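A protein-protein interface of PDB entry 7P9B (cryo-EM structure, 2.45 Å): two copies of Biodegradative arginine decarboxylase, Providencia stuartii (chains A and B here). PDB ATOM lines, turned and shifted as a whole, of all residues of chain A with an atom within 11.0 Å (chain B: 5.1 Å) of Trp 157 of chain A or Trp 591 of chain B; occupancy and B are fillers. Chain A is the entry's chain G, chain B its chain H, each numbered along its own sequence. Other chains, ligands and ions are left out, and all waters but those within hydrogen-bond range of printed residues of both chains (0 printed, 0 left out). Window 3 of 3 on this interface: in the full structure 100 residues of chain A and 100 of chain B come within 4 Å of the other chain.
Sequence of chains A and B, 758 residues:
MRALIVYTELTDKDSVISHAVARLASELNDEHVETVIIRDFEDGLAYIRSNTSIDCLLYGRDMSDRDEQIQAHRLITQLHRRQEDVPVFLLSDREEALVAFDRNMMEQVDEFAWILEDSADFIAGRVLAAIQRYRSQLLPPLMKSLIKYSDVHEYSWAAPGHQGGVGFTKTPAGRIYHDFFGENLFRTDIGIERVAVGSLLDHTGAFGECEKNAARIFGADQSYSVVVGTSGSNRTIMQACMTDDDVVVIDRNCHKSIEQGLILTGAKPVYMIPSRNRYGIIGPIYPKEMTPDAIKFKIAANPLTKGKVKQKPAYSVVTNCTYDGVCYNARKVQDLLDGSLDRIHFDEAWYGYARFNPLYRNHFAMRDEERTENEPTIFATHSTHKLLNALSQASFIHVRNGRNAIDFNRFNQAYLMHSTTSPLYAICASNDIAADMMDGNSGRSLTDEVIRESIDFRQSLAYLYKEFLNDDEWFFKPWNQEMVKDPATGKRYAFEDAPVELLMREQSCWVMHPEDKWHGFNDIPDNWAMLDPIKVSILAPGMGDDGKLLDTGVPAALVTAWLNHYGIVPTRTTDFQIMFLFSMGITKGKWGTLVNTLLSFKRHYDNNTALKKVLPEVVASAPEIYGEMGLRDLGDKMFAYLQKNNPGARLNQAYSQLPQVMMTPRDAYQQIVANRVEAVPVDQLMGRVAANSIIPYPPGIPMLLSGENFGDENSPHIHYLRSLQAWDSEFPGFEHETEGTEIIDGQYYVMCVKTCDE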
ATOM      1  N   TYR A 149     -18.388  18.593   3.165  1.00  0.00           N
ATOM      2  CA  TYR A 149     -18.051  17.754   4.305  1.00  0.00           C
ATOM      3  C   TYR A 149     -19.271  17.028   4.856  1.00  0.00           C
ATOM      4  O   TYR A 149     -19.126  16.023   5.556  1.00  0.00           O
ATOM      5  CB  TYR A 149     -17.391  18.595   5.391  1.00  0.00           C
ATOM      6  CG  TYR A 149     -16.925  17.775   6.560  1.00  0.00           C
ATOM      7  CD1 TYR A 149     -15.741  17.060   6.498  1.00  0.00           C
ATOM      8  CD2 TYR A 149     -17.682  17.689   7.715  1.00  0.00           C
ATOM      9  CE1 TYR A 149     -15.317  16.296   7.559  1.00  0.00           C
ATOM     10  CE2 TYR A 149     -17.267  16.925   8.779  1.00  0.00           C
ATOM     11  CZ  TYR A 149     -16.083  16.232   8.695  1.00  0.00           C
ATOM     12  OH  TYR A 149     -15.655  15.462   9.747  1.00  0.00           O
ATOM     13  N   VAL A 152     -19.625  13.254   4.653  1.00  0.00           N
ATOM     14  CA  VAL A 152     -18.810  12.381   5.488  1.00  0.00           C
ATOM     15  C   VAL A 152     -19.622  11.931   6.697  1.00  0.00           C
ATOM     16  O   VAL A 152     -20.015  12.748   7.539  1.00  0.00           O
ATOM     17  CB  VAL A 152     -17.528  13.113   5.906  1.00  0.00           C
ATOM     18  CG1 VAL A 152     -16.724  12.289   6.883  1.00  0.00           C
ATOM     19  CG2 VAL A 152     -16.703  13.457   4.675  1.00  0.00           C
ATOM     20  N   HIS A 153     -19.856  10.618   6.800  1.00  0.00           N
ATOM     21  CA  HIS A 153     -20.838  10.074   7.731  1.00  0.00           C
ATOM     22  C   HIS A 153     -20.246   9.295   8.900  1.00  0.00           C
ATOM     23  O   HIS A 153     -21.003   8.889   9.786  1.00  0.00           O
ATOM     24  CB  HIS A 153     -21.817   9.148   7.005  1.00  0.00           C
ATOM     25  CG  HIS A 153     -22.642   9.826   5.963  1.00  0.00           C
ATOM     26  ND1 HIS A 153     -23.693  10.660   6.273  1.00  0.00           N
ATOM     27  CD2 HIS A 153     -22.589   9.773   4.612  1.00  0.00           C
ATOM     28  CE1 HIS A 153     -24.243  11.103   5.157  1.00  0.00           C
ATOM     29  NE2 HIS A 153     -23.593  10.581   4.135  1.00  0.00           N
ATOM     30  N   GLU A 154     -18.943   9.035   8.922  1.00  0.00           N
ATOM     31  CA  GLU A 154     -18.429   8.080   9.893  1.00  0.00           C
ATOM     32  C   GLU A 154     -18.523   8.617  11.314  1.00  0.00           C
ATOM     33  O   GLU A 154     -18.553   9.826  11.552  1.00  0.00           O
ATOM     34  CB  GLU A 154     -16.979   7.691   9.597  1.00  0.00           C
ATOM     35  CG  GLU A 154     -15.948   8.777   9.835  1.00  0.00           C
ATOM     36  CD  GLU A 154     -15.569   9.507   8.567  1.00  0.00           C
ATOM     37  OE1 GLU A 154     -16.272   9.337   7.550  1.00  0.00           O
ATOM     38  OE2 GLU A 154     -14.561  10.241   8.584  1.00  0.00           O
ATOM     39  N   TYR A 155     -18.581   7.689  12.262  1.00  0.00           N
ATOM     40  CA  TYR A 155     -18.564   8.017  13.681  1.00  0.00           C
ATOM     41  C   TYR A 155     -17.216   8.615  14.045  1.00  0.00           C
ATOM     42  O   TYR A 155     -16.194   7.927  14.011  1.00  0.00           O
ATOM     43  CB  TYR A 155     -18.836   6.767  14.508  1.00  0.00           C
ATOM     44  CG  TYR A 155     -18.810   7.014  15.995  1.00  0.00           C
ATOM     45  CD1 TYR A 155     -19.899   7.552  16.646  1.00  0.00           C
ATOM     46  CD2 TYR A 155     -17.686   6.730  16.740  1.00  0.00           C
ATOM     47  CE1 TYR A 155     -19.873   7.785  17.997  1.00  0.00           C
ATOM     48  CE2 TYR A 155     -17.656   6.965  18.085  1.00  0.00           C
ATOM     49  CZ  TYR A 155     -18.752   7.493  18.710  1.00  0.00           C
ATOM     50  OH  TYR A 155     -18.719   7.728  20.057  1.00  0.00           O
ATOM     51  N   SER A 156     -17.199   9.900  14.370  1.00  0.00           N
ATOM     52  CA  SER A 156     -16.056  10.465  15.058  1.00  0.00           C
ATOM     53  C   SER A 156     -16.175  10.162  16.541  1.00  0.00           C
ATOM     54  O   SER A 156     -17.269   9.974  17.071  1.00  0.00           O
ATOM     55  CB  SER A 156     -15.978  11.969  14.834  1.00  0.00           C
ATOM     56  OG  SER A 156     -17.070  12.623  15.446  1.00  0.00           O
ATOM     57  N   TRP A 157     -15.041  10.115  17.219  1.00  0.00           N
ATOM     58  CA  TRP A 157     -15.006   9.701  18.617  1.00  0.00           C
ATOM     59  C   TRP A 157     -14.971  10.905  19.538  1.00  0.00           C
ATOM     60  O   TRP A 157     -14.288  10.906  20.561  1.00  0.00           O
ATOM     61  CB  TRP A 157     -13.817   8.777  18.835  1.00  0.00           C
ATOM     62  CG  TRP A 157     -13.990   7.527  18.038  1.00  0.00           C
ATOM     63  CD1 TRP A 157     -13.670   7.349  16.730  1.00  0.00           C
ATOM     64  CD2 TRP A 157     -14.513   6.278  18.492  1.00  0.00           C
ATOM     65  NE1 TRP A 157     -13.979   6.079  16.331  1.00  0.00           N
ATOM     66  CE2 TRP A 157     -14.496   5.398  17.398  1.00  0.00           C
ATOM     67  CE3 TRP A 157     -15.004   5.822  19.715  1.00  0.00           C
ATOM     68  CZ2 TRP A 157     -14.948   4.090  17.490  1.00  0.00           C
ATOM     69  CZ3 TRP A 157     -15.456   4.526  19.800  1.00  0.00           C
ATOM     70  CH2 TRP A 157     -15.423   3.674  18.697  1.00  0.00           C
ATOM     71  N   ALA A 158     -15.705  11.952  19.163  1.00  0.00           N
ATOM     72  CA  ALA A 158     -15.680  13.230  19.852  1.00  0.00           C
ATOM     73  C   ALA A 158     -17.038  13.906  19.718  1.00  0.00           C
ATOM     74  O   ALA A 158     -17.888  13.491  18.932  1.00  0.00           O
ATOM     75  CB  ALA A 158     -14.570  14.127  19.300  1.00  0.00           C
ATOM     76  N   ALA A 159     -17.230  14.971  20.496  1.00  0.00           N
ATOM     77  CA  ALA A 159     -18.482  15.708  20.501  1.00  0.00           C
ATOM     78  C   ALA A 159     -18.699  16.419  19.164  1.00  0.00           C
ATOM     79  O   ALA A 159     -17.746  16.692  18.437  1.00  0.00           O
ATOM     80  CB  ALA A 159     -18.488  16.713  21.646  1.00  0.00           C
ATOM     81  N   PRO A 160     -19.959  16.732  18.812  1.00  0.00           N
ATOM     82  CA  PRO A 160     -21.224  16.503  19.518  1.00  0.00           C
ATOM     83  C   PRO A 160     -21.650  15.043  19.565  1.00  0.00           C
ATOM     84  O   PRO A 160     -21.372  14.278  18.652  1.00  0.00           O
ATOM     85  CB  PRO A 160     -22.229  17.330  18.713  1.00  0.00           C
ATOM     86  CG  PRO A 160     -21.652  17.414  17.376  1.00  0.00           C
ATOM     87  CD  PRO A 160     -20.172  17.463  17.554  1.00  0.00           C
ATOM     88  N   GLY A 161     -22.347  14.681  20.638  1.00  0.00           N
ATOM     89  CA  GLY A 161     -22.661  13.289  20.881  1.00  0.00           C
ATOM     90  C   GLY A 161     -23.718  12.713  19.965  1.00  0.00           C
ATOM     91  O   GLY A 161     -23.804  11.495  19.817  1.00  0.00           O
ATOM     92  N   HIS A 162     -24.542  13.560  19.345  1.00  0.00           N
ATOM     93  CA  HIS A 162     -25.579  13.016  18.476  1.00  0.00           C
ATOM     94  C   HIS A 162     -25.011  12.438  17.189  1.00  0.00           C
ATOM     95  O   HIS A 162     -25.698  11.656  16.532  1.00  0.00           O
ATOM     96  CB  HIS A 162     -26.656  14.061  18.168  1.00  0.00           C
ATOM     97  CG  HIS A 162     -26.169  15.263  17.421  1.00  0.00           C
ATOM     98  ND1 HIS A 162     -26.040  15.285  16.051  1.00  0.00           N
ATOM     99  CD2 HIS A 162     -25.839  16.501  17.847  1.00  0.00           C
ATOM    100  CE1 HIS A 162     -25.617  16.475  15.669  1.00  0.00           C
ATOM    101  NE2 HIS A 162     -25.491  17.232  16.740  1.00  0.00           N
ATOM    102  N   GLN A 163     -23.776  12.783  16.829  1.00  0.00           N
ATOM    103  CA  GLN A 163     -23.048  12.138  15.737  1.00  0.00           C
ATOM    104  C   GLN A 163     -23.801  12.248  14.413  1.00  0.00           C
ATOM    105  O   GLN A 163     -24.211  11.257  13.818  1.00  0.00           O
ATOM    106  CB  GLN A 163     -22.752  10.672  16.070  1.00  0.00           C
ATOM    107  CG  GLN A 163     -21.842  10.467  17.250  1.00  0.00           C
ATOM    108  CD  GLN A 163     -20.437  10.936  16.992  1.00  0.00           C
ATOM    109  OE1 GLN A 163     -19.912  10.786  15.894  1.00  0.00           O
ATOM    110  NE2 GLN A 163     -19.810  11.498  18.008  1.00  0.00           N
ATOM    111  N   GLY A 164     -23.965  13.482  13.954  1.00  0.00           N
ATOM    112  CA  GLY A 164     -24.667  13.708  12.712  1.00  0.00           C
ATOM    113  C   GLY A 164     -26.131  13.346  12.754  1.00  0.00           C
ATOM    114  O   GLY A 164     -26.707  13.009  11.720  1.00  0.00           O
ATOM    115  N   ILE A 190     -20.783  19.678  13.267  1.00  0.00           N
ATOM    116  CA  ILE A 190     -19.605  18.822  13.195  1.00  0.00           C
ATOM    117  C   ILE A 190     -18.609  19.069  14.312  1.00  0.00           C
ATOM    118  O   ILE A 190     -17.777  18.188  14.576  1.00  0.00           O
ATOM    119  CB  ILE A 190     -18.901  18.955  11.831  1.00  0.00           C
ATOM    120  CG1 ILE A 190     -18.477  20.399  11.594  1.00  0.00           C
ATOM    121  CG2 ILE A 190     -19.802  18.488  10.724  1.00  0.00           C
ATOM    122  CD1 ILE A 190     -17.583  20.576  10.416  1.00  0.00           C
ATOM    123  N   GLY A 191     -18.654  20.213  14.973  1.00  0.00           N
ATOM    124  CA  GLY A 191     -17.658  20.539  15.967  1.00  0.00           C
ATOM    125  C   GLY A 191     -16.474  21.265  15.362  1.00  0.00           C
ATOM    126  O   GLY A 191     -16.284  21.322  14.148  1.00  0.00           O
ATOM    127  N   GLU A 193     -13.282  20.697  15.575  1.00  0.00           N
ATOM    128  CA  GLU A 193     -12.064  19.921  15.387  1.00  0.00           C
ATOM    129  C   GLU A 193     -12.042  19.173  14.061  1.00  0.00           C
ATOM    130  O   GLU A 193     -11.599  18.023  14.010  1.00  0.00           O
ATOM    131  CB  GLU A 193     -11.869  18.943  16.544  1.00  0.00           C
ATOM    132  CG  GLU A 193     -11.556  19.612  17.864  1.00  0.00           C
ATOM    133  CD  GLU A 193     -10.216  20.328  17.856  1.00  0.00           C
ATOM    134  OE1 GLU A 193      -9.287  19.865  17.160  1.00  0.00           O
ATOM    135  OE2 GLU A 193     -10.094  21.359  18.548  1.00  0.00           O
ATOM    136  N   ARG A 194     -12.515  19.796  12.990  1.00  0.00           N
ATOM    137  CA  ARG A 194     -12.355  19.270  11.641  1.00  0.00           C
ATOM    138  C   ARG A 194     -11.529  20.267  10.840  1.00  0.00           C
ATOM    139  O   ARG A 194     -11.985  21.374  10.548  1.00  0.00           O
ATOM    140  CB  ARG A 194     -13.702  18.995  10.983  1.00  0.00           C
ATOM    141  CG  ARG A 194     -14.258  17.631  11.306  1.00  0.00           C
ATOM    142  CD  ARG A 194     -14.913  17.558  12.665  1.00  0.00           C
ATOM    143  NE  ARG A 194     -15.384  16.204  12.951  1.00  0.00           N
ATOM    144  CZ  ARG A 194     -16.550  15.712  12.538  1.00  0.00           C
ATOM    145  NH1 ARG A 194     -17.355  16.453  11.799  1.00  0.00           N
ATOM    146  NH2 ARG A 194     -16.901  14.471  12.841  1.00  0.00           N
ATOM    147  N   GLU B 453     -21.438  -0.726  25.432  1.00  0.00           N
ATOM    148  CA  GLU B 453     -20.538  -0.570  24.296  1.00  0.00           C
ATOM    149  C   GLU B 453     -19.108  -0.284  24.754  1.00  0.00           C
ATOM    150  O   GLU B 453     -18.145  -0.914  24.286  1.00  0.00           O
ATOM    151  CB  GLU B 453     -21.077   0.559  23.423  1.00  0.00           C
ATOM    152  CG  GLU B 453     -20.417   0.796  22.105  1.00  0.00           C
ATOM    153  CD  GLU B 453     -20.729  -0.278  21.086  1.00  0.00           C
ATOM    154  OE1 GLU B 453     -21.707  -1.030  21.283  1.00  0.00           O
ATOM    155  OE2 GLU B 453     -20.022  -0.323  20.058  1.00  0.00           O
ATOM    156  N   ASP B 456     -17.505  -3.342  26.422  1.00  0.00           N
ATOM    157  CA  ASP B 456     -17.037  -4.301  25.431  1.00  0.00           C
ATOM    158  C   ASP B 456     -15.702  -3.887  24.854  1.00  0.00           C
ATOM    159  O   ASP B 456     -14.792  -4.711  24.732  1.00  0.00           O
ATOM    160  CB  ASP B 456     -18.038  -4.458  24.301  1.00  0.00           C
ATOM    161  CG  ASP B 456     -19.251  -5.197  24.717  1.00  0.00           C
ATOM    162  OD1 ASP B 456     -19.170  -6.010  25.655  1.00  0.00           O
ATOM    163  OD2 ASP B 456     -20.300  -4.970  24.100  1.00  0.00           O
ATOM    164  N   PHE B 457     -15.574  -2.619  24.469  1.00  0.00           N
ATOM    165  CA  PHE B 457     -14.280  -2.164  23.976  1.00  0.00           C
ATOM    166  C   PHE B 457     -13.184  -2.378  25.014  1.00  0.00           C
ATOM    167  O   PHE B 457     -12.101  -2.878  24.693  1.00  0.00           O
ATOM    168  CB  PHE B 457     -14.349  -0.702  23.556  1.00  0.00           C
ATOM    169  CG  PHE B 457     -13.037  -0.159  23.103  1.00  0.00           C
ATOM    170  CD1 PHE B 457     -12.464  -0.597  21.930  1.00  0.00           C
ATOM    171  CD2 PHE B 457     -12.376   0.791  23.842  1.00  0.00           C
ATOM    172  CE1 PHE B 457     -11.259  -0.112  21.514  1.00  0.00           C
ATOM    173  CE2 PHE B 457     -11.171   1.285  23.423  1.00  0.00           C
ATOM    174  CZ  PHE B 457     -10.613   0.833  22.260  1.00  0.00           C
ATOM    175  N   SER B 460     -12.347  -6.181  25.472  1.00  0.00           N
ATOM    176  CA  SER B 460     -11.669  -6.722  24.302  1.00  0.00           C
ATOM    177  C   SER B 460     -10.236  -6.218  24.215  1.00  0.00           C
ATOM    178  O   SER B 460      -9.320  -6.979  23.888  1.00  0.00           O
ATOM    179  CB  SER B 460     -12.451  -6.364  23.046  1.00  0.00           C
ATOM    180  OG  SER B 460     -13.729  -6.957  23.085  1.00  0.00           O
ATOM    181  N   ILE B 568     -10.108   9.228  12.765  1.00  0.00           N
ATOM    182  CA  ILE B 568     -10.399   9.063  14.184  1.00  0.00           C
ATOM    183  C   ILE B 568      -9.652  10.133  14.962  1.00  0.00           C
ATOM    184  O   ILE B 568      -8.434  10.040  15.152  1.00  0.00           O
ATOM    185  CB  ILE B 568     -10.007   7.659  14.656  1.00  0.00           C
ATOM    186  CG1 ILE B 568     -10.737   6.605  13.834  1.00  0.00           C
ATOM    187  CG2 ILE B 568     -10.338   7.481  16.115  1.00  0.00           C
ATOM    188  CD1 ILE B 568     -10.183   5.223  14.003  1.00  0.00           C
ATOM    189  N   VAL B 569     -10.369  11.152  15.412  1.00  0.00           N
ATOM    190  CA  VAL B 569      -9.746  12.261  16.126  1.00  0.00           C
ATOM    191  C   VAL B 569      -9.991  12.110  17.625  1.00  0.00           C
ATOM    192  O   VAL B 569     -11.135  12.203  18.089  1.00  0.00           O
ATOM    193  CB  VAL B 569     -10.240  13.609  15.573  1.00  0.00           C
ATOM    194  CG1 VAL B 569     -11.759  13.711  15.634  1.00  0.00           C
ATOM    195  CG2 VAL B 569      -9.588  14.767  16.313  1.00  0.00           C
ATOM    196  N   THR B 571     -10.164  12.935  21.649  1.00  0.00           N
ATOM    197  CA  THR B 571     -10.483  14.125  22.428  1.00  0.00           C
ATOM    198  C   THR B 571      -9.285  14.585  23.251  1.00  0.00           C
ATOM    199  O   THR B 571      -8.926  15.765  23.235  1.00  0.00           O
ATOM    200  CB  THR B 571     -11.679  13.849  23.340  1.00  0.00           C
ATOM    201  OG1 THR B 571     -12.828  13.525  22.546  1.00  0.00           O
ATOM    202  CG2 THR B 571     -11.987  15.055  24.200  1.00  0.00           C
ATOM    203  N   PHE B 580     -10.790   8.214  23.997  1.00  0.00           N
ATOM    204  CA  PHE B 580     -11.878   8.092  23.044  1.00  0.00           C
ATOM    205  C   PHE B 580     -13.192   8.293  23.776  1.00  0.00           C
ATOM    206  O   PHE B 580     -13.317   7.961  24.959  1.00  0.00           O
ATOM    207  CB  PHE B 580     -11.873   6.725  22.380  1.00  0.00           C
ATOM    208  CG  PHE B 580     -10.633   6.443  21.610  1.00  0.00           C
ATOM    209  CD1 PHE B 580     -10.484   6.905  20.324  1.00  0.00           C
ATOM    210  CD2 PHE B 580      -9.601   5.735  22.184  1.00  0.00           C
ATOM    211  CE1 PHE B 580      -9.342   6.652  19.625  1.00  0.00           C
ATOM    212  CE2 PHE B 580      -8.457   5.485  21.485  1.00  0.00           C
ATOM    213  CZ  PHE B 580      -8.327   5.940  20.204  1.00  0.00           C
ATOM    214  N   LEU B 581     -14.169   8.832  23.073  1.00  0.00           N
ATOM    215  CA  LEU B 581     -15.448   9.168  23.667  1.00  0.00           C
ATOM    216  C   LEU B 581     -16.523   8.285  23.058  1.00  0.00           C
ATOM    217  O   LEU B 581     -16.662   8.234  21.836  1.00  0.00           O
ATOM    218  CB  LEU B 581     -15.762  10.641  23.427  1.00  0.00           C
ATOM    219  CG  LEU B 581     -16.964  11.263  24.114  1.00  0.00           C
ATOM    220  CD1 LEU B 581     -16.736  11.262  25.604  1.00  0.00           C
ATOM    221  CD2 LEU B 581     -17.161  12.665  23.597  1.00  0.00           C
ATOM    222  N   PHE B 582     -17.272   7.583  23.905  1.00  0.00           N
ATOM    223  CA  PHE B 582     -18.448   6.859  23.448  1.00  0.00           C
ATOM    224  C   PHE B 582     -19.666   7.685  23.833  1.00  0.00           C
ATOM    225  O   PHE B 582     -19.863   7.995  25.009  1.00  0.00           O
ATOM    226  CB  PHE B 582     -18.568   5.445  24.023  1.00  0.00           C
ATOM    227  CG  PHE B 582     -17.452   4.504  23.641  1.00  0.00           C
ATOM    228  CD1 PHE B 582     -16.190   4.955  23.317  1.00  0.00           C
ATOM    229  CD2 PHE B 582     -17.732   3.173  23.430  1.00  0.00           C
ATOM    230  CE1 PHE B 582     -15.200   4.082  22.946  1.00  0.00           C
ATOM    231  CE2 PHE B 582     -16.756   2.299  23.027  1.00  0.00           C
ATOM    232  CZ  PHE B 582     -15.489   2.753  22.784  1.00  0.00           C
ATOM    233  N   ILE B 586     -23.262   6.775  19.125  1.00  0.00           N
ATOM    234  CA  ILE B 586     -22.495   5.645  18.621  1.00  0.00           C
ATOM    235  C   ILE B 586     -23.446   4.498  18.322  1.00  0.00           C
ATOM    236  O   ILE B 586     -24.519   4.376  18.918  1.00  0.00           O
ATOM    237  CB  ILE B 586     -21.401   5.224  19.624  1.00  0.00           C
ATOM    238  CG1 ILE B 586     -20.339   4.377  18.935  1.00  0.00           C
ATOM    239  CG2 ILE B 586     -21.977   4.393  20.732  1.00  0.00           C
ATOM    240  CD1 ILE B 586     -19.138   4.118  19.790  1.00  0.00           C
ATOM    241  N   GLY B 589     -21.240  -2.146  18.173  1.00  0.00           N
ATOM    242  CA  GLY B 589     -20.157  -2.840  17.516  1.00  0.00           C
ATOM    243  C   GLY B 589     -19.178  -1.956  16.787  1.00  0.00           C
ATOM    244  O   GLY B 589     -18.227  -2.473  16.197  1.00  0.00           O
ATOM    245  N   LYS B 590     -19.380  -0.641  16.810  1.00  0.00           N
ATOM    246  CA  LYS B 590     -18.489   0.268  16.104  1.00  0.00           C
ATOM    247  C   LYS B 590     -17.067   0.212  16.647  1.00  0.00           C
ATOM    248  O   LYS B 590     -16.109   0.337  15.879  1.00  0.00           O
ATOM    249  CB  LYS B 590     -19.045   1.689  16.182  1.00  0.00           C
ATOM    250  CG  LYS B 590     -18.183   2.731  15.526  1.00  0.00           C
ATOM    251  CD  LYS B 590     -18.164   2.563  14.031  1.00  0.00           C
ATOM    252  CE  LYS B 590     -17.312   3.626  13.375  1.00  0.00           C
ATOM    253  NZ  LYS B 590     -17.225   3.418  11.915  1.00  0.00           N
ATOM    254  N   TRP B 591     -16.908  -0.003  17.952  1.00  0.00           N
ATOM    255  CA  TRP B 591     -15.584  -0.047  18.558  1.00  0.00           C
ATOM    256  C   TRP B 591     -14.668  -1.075  17.915  1.00  0.00           C
ATOM    257  O   TRP B 591     -13.446  -0.906  17.979  1.00  0.00           O
ATOM    258  CB  TRP B 591     -15.695  -0.324  20.056  1.00  0.00           C
ATOM    259  CG  TRP B 591     -16.388  -1.603  20.395  1.00  0.00           C
ATOM    260  CD1 TRP B 591     -17.702  -1.765  20.665  1.00  0.00           C
ATOM    261  CD2 TRP B 591     -15.795  -2.898  20.489  1.00  0.00           C
ATOM    262  NE1 TRP B 591     -17.973  -3.077  20.928  1.00  0.00           N
ATOM    263  CE2 TRP B 591     -16.815  -3.797  20.824  1.00  0.00           C
ATOM    264  CE3 TRP B 591     -14.500  -3.385  20.324  1.00  0.00           C
ATOM    265  CZ2 TRP B 591     -16.584  -5.150  20.998  1.00  0.00           C
ATOM    266  CZ3 TRP B 591     -14.275  -4.722  20.491  1.00  0.00           C
ATOM    267  CH2 TRP B 591     -15.308  -5.593  20.826  1.00  0.00           C
ATOM    268  N   GLY B 592     -15.214  -2.128  17.309  1.00  0.00           N
ATOM    269  CA  GLY B 592     -14.377  -3.078  16.600  1.00  0.00           C
ATOM    270  C   GLY B 592     -13.485  -2.405  15.581  1.00  0.00           C
ATOM    271  O   GLY B 592     -12.288  -2.692  15.506  1.00  0.00           O
ATOM    272  N   THR B 593     -14.052  -1.479  14.801  1.00  0.00           N
ATOM    273  CA  THR B 593     -13.254  -0.669  13.889  1.00  0.00           C
ATOM    274  C   THR B 593     -12.022  -0.124  14.583  1.00  0.00           C
ATOM    275  O   THR B 593     -10.895  -0.322  14.121  1.00  0.00           O
ATOM    276  CB  THR B 593     -14.088   0.488  13.351  1.00  0.00           C
ATOM    277  OG1 THR B 593     -15.249  -0.020  12.693  1.00  0.00           O
ATOM    278  CG2 THR B 593     -13.289   1.300  12.367  1.00  0.00           C
ATOM    279  N   LEU B 594     -12.224   0.527  15.725  1.00  0.00           N
ATOM    280  CA  LEU B 594     -11.119   1.110  16.464  1.00  0.00           C
ATOM    281  C   LEU B 594     -10.077   0.054  16.798  1.00  0.00           C
ATOM    282  O   LEU B 594      -8.887   0.242  16.523  1.00  0.00           O
ATOM    283  CB  LEU B 594     -11.661   1.785  17.719  1.00  0.00           C
ATOM    284  CG  LEU B 594     -10.715   2.634  18.543  1.00  0.00           C
ATOM    285  CD1 LEU B 594     -10.190   3.745  17.679  1.00  0.00           C
ATOM    286  CD2 LEU B 594     -11.470   3.195  19.718  1.00  0.00           C
ATOM    287  N   VAL B 595     -10.517  -1.089  17.327  1.00  0.00           N
ATOM    288  CA  VAL B 595      -9.593  -2.188  17.591  1.00  0.00           C
ATOM    289  C   VAL B 595      -8.801  -2.520  16.340  1.00  0.00           C
ATOM    290  O   VAL B 595      -7.564  -2.542  16.361  1.00  0.00           O
ATOM    291  CB  VAL B 595     -10.353  -3.411  18.126  1.00  0.00           C
ATOM    292  CG1 VAL B 595      -9.461  -4.617  18.130  1.00  0.00           C
ATOM    293  CG2 VAL B 595     -10.842  -3.147  19.523  1.00  0.00           C
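The backbone carbonyl oxygen (O) of Trp 157 of chain A lies close to the backbone NH (N) of Leu 581 of chain B (3.3 Å). The side-chain hydroxyl of Tyr 155 of chain A lies within hydrogen-bond range of the backbone carbonyl oxygen of Leu 581 of chain B (2.8 Å).
The side-chain hydroxyl (OG1) of Thr 593 of chain B sits close to the backbone carbonyl oxygen (O) of Lys 590 of chain B. The backbone NH (N) of Lys 590 of chain B sits at hydrogen-bond distance from the side-chain carboxylate (OE2) of Glu 453 of chain B (3.3 Å). The backbone carbonyl oxygen (O) of Ala 158 of chain A is in hydrogen-bond range of the side-chain amide nitrogen (NE2) of Gln 163 of chain A, 2.9 Å away.
Of the printed residues of chain B, Tyr 155 of chain A touches Leu 581 (2.8 Å), Phe 582 (3.5 Å), Ile 586 (3.4 Å) and Lys 590 (3.7 Å). Trp 157 of chain A touches just these residues of chain B: Ile 568, Thr 571, Leu 581, Phe 582, Ile 586 and Trp 591. Of the printed residues of chain B, Ala 159 of chain A touches Leu 581 (3.9 Å). No residue of chain A comes within 4 Å of Glu 453 of chain B. No residue of chain A comes within 4 Å of Asp 456 of chain B. Phe 457 of chain B touches none of the printed residues of chain A. Of chain A, only Tyr 155, Trp 157 and Ala 159 come within 4 Å of Leu 581 of chain B. Of the printed residues of chain A, Phe 582 of chain B touches Tyr 155 and Trp 157. Of the printed residues of chain A, Ile 586 of chain B touches Tyr 155 and Trp 157. No residue of chain A comes within 4 Å of Gly 589 of chain B. No residue of chain A comes within 4 Å of Val 595 of chain B. The nearest printed residue of chain B that does not touch Trp 157 of chain A is Lys 590 of chain B (4.02 Å).
CA of Phe 582 of chain B touches OH of Tyr 155 of chain A, 3.5 Å away. Tyr 155 of chain A touches Ile 586 of chain B. Tyr 155 of chain A touches Lys 590 of chain B (CB to CE, 3.7 Å). Trp 157 of chain A touches Ile 568 of chain B. Thr 571 of chain B touches Trp 157 of chain A. CE1 of Phe 582 of chain B touches CZ3 of Trp 157 of chain A, at 3.2 Å. Trp 157 of chain A touches Ile 586 of chain B. Trp 157 of chain A touches Trp 591 of chain B (CH2 to CA, 3.7 Å). Ala 159 of chain A touches Leu 581 of chain B.
Of the 18 printed residues of chain A, 4 touch a printed residue of chain B. Printed residues of chain A that touch a printed residue of chain B: Tyr 155, Trp 157, Ala 158 and Ala 159. Hydrophobic or aromatic side chains of chain A that line the printed part of chain B: Tyr 155, Trp 157 and Ala 158. Among the printed residues, no Asp or Glu carboxylate lies within 4 Å of a Lys or Arg side-chain nitrogen of the other chain.
No position is printed for both chains. Of the 12 pairs that touch across the chains among the printed residues, none has its exchanged pair printed and touching as well.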
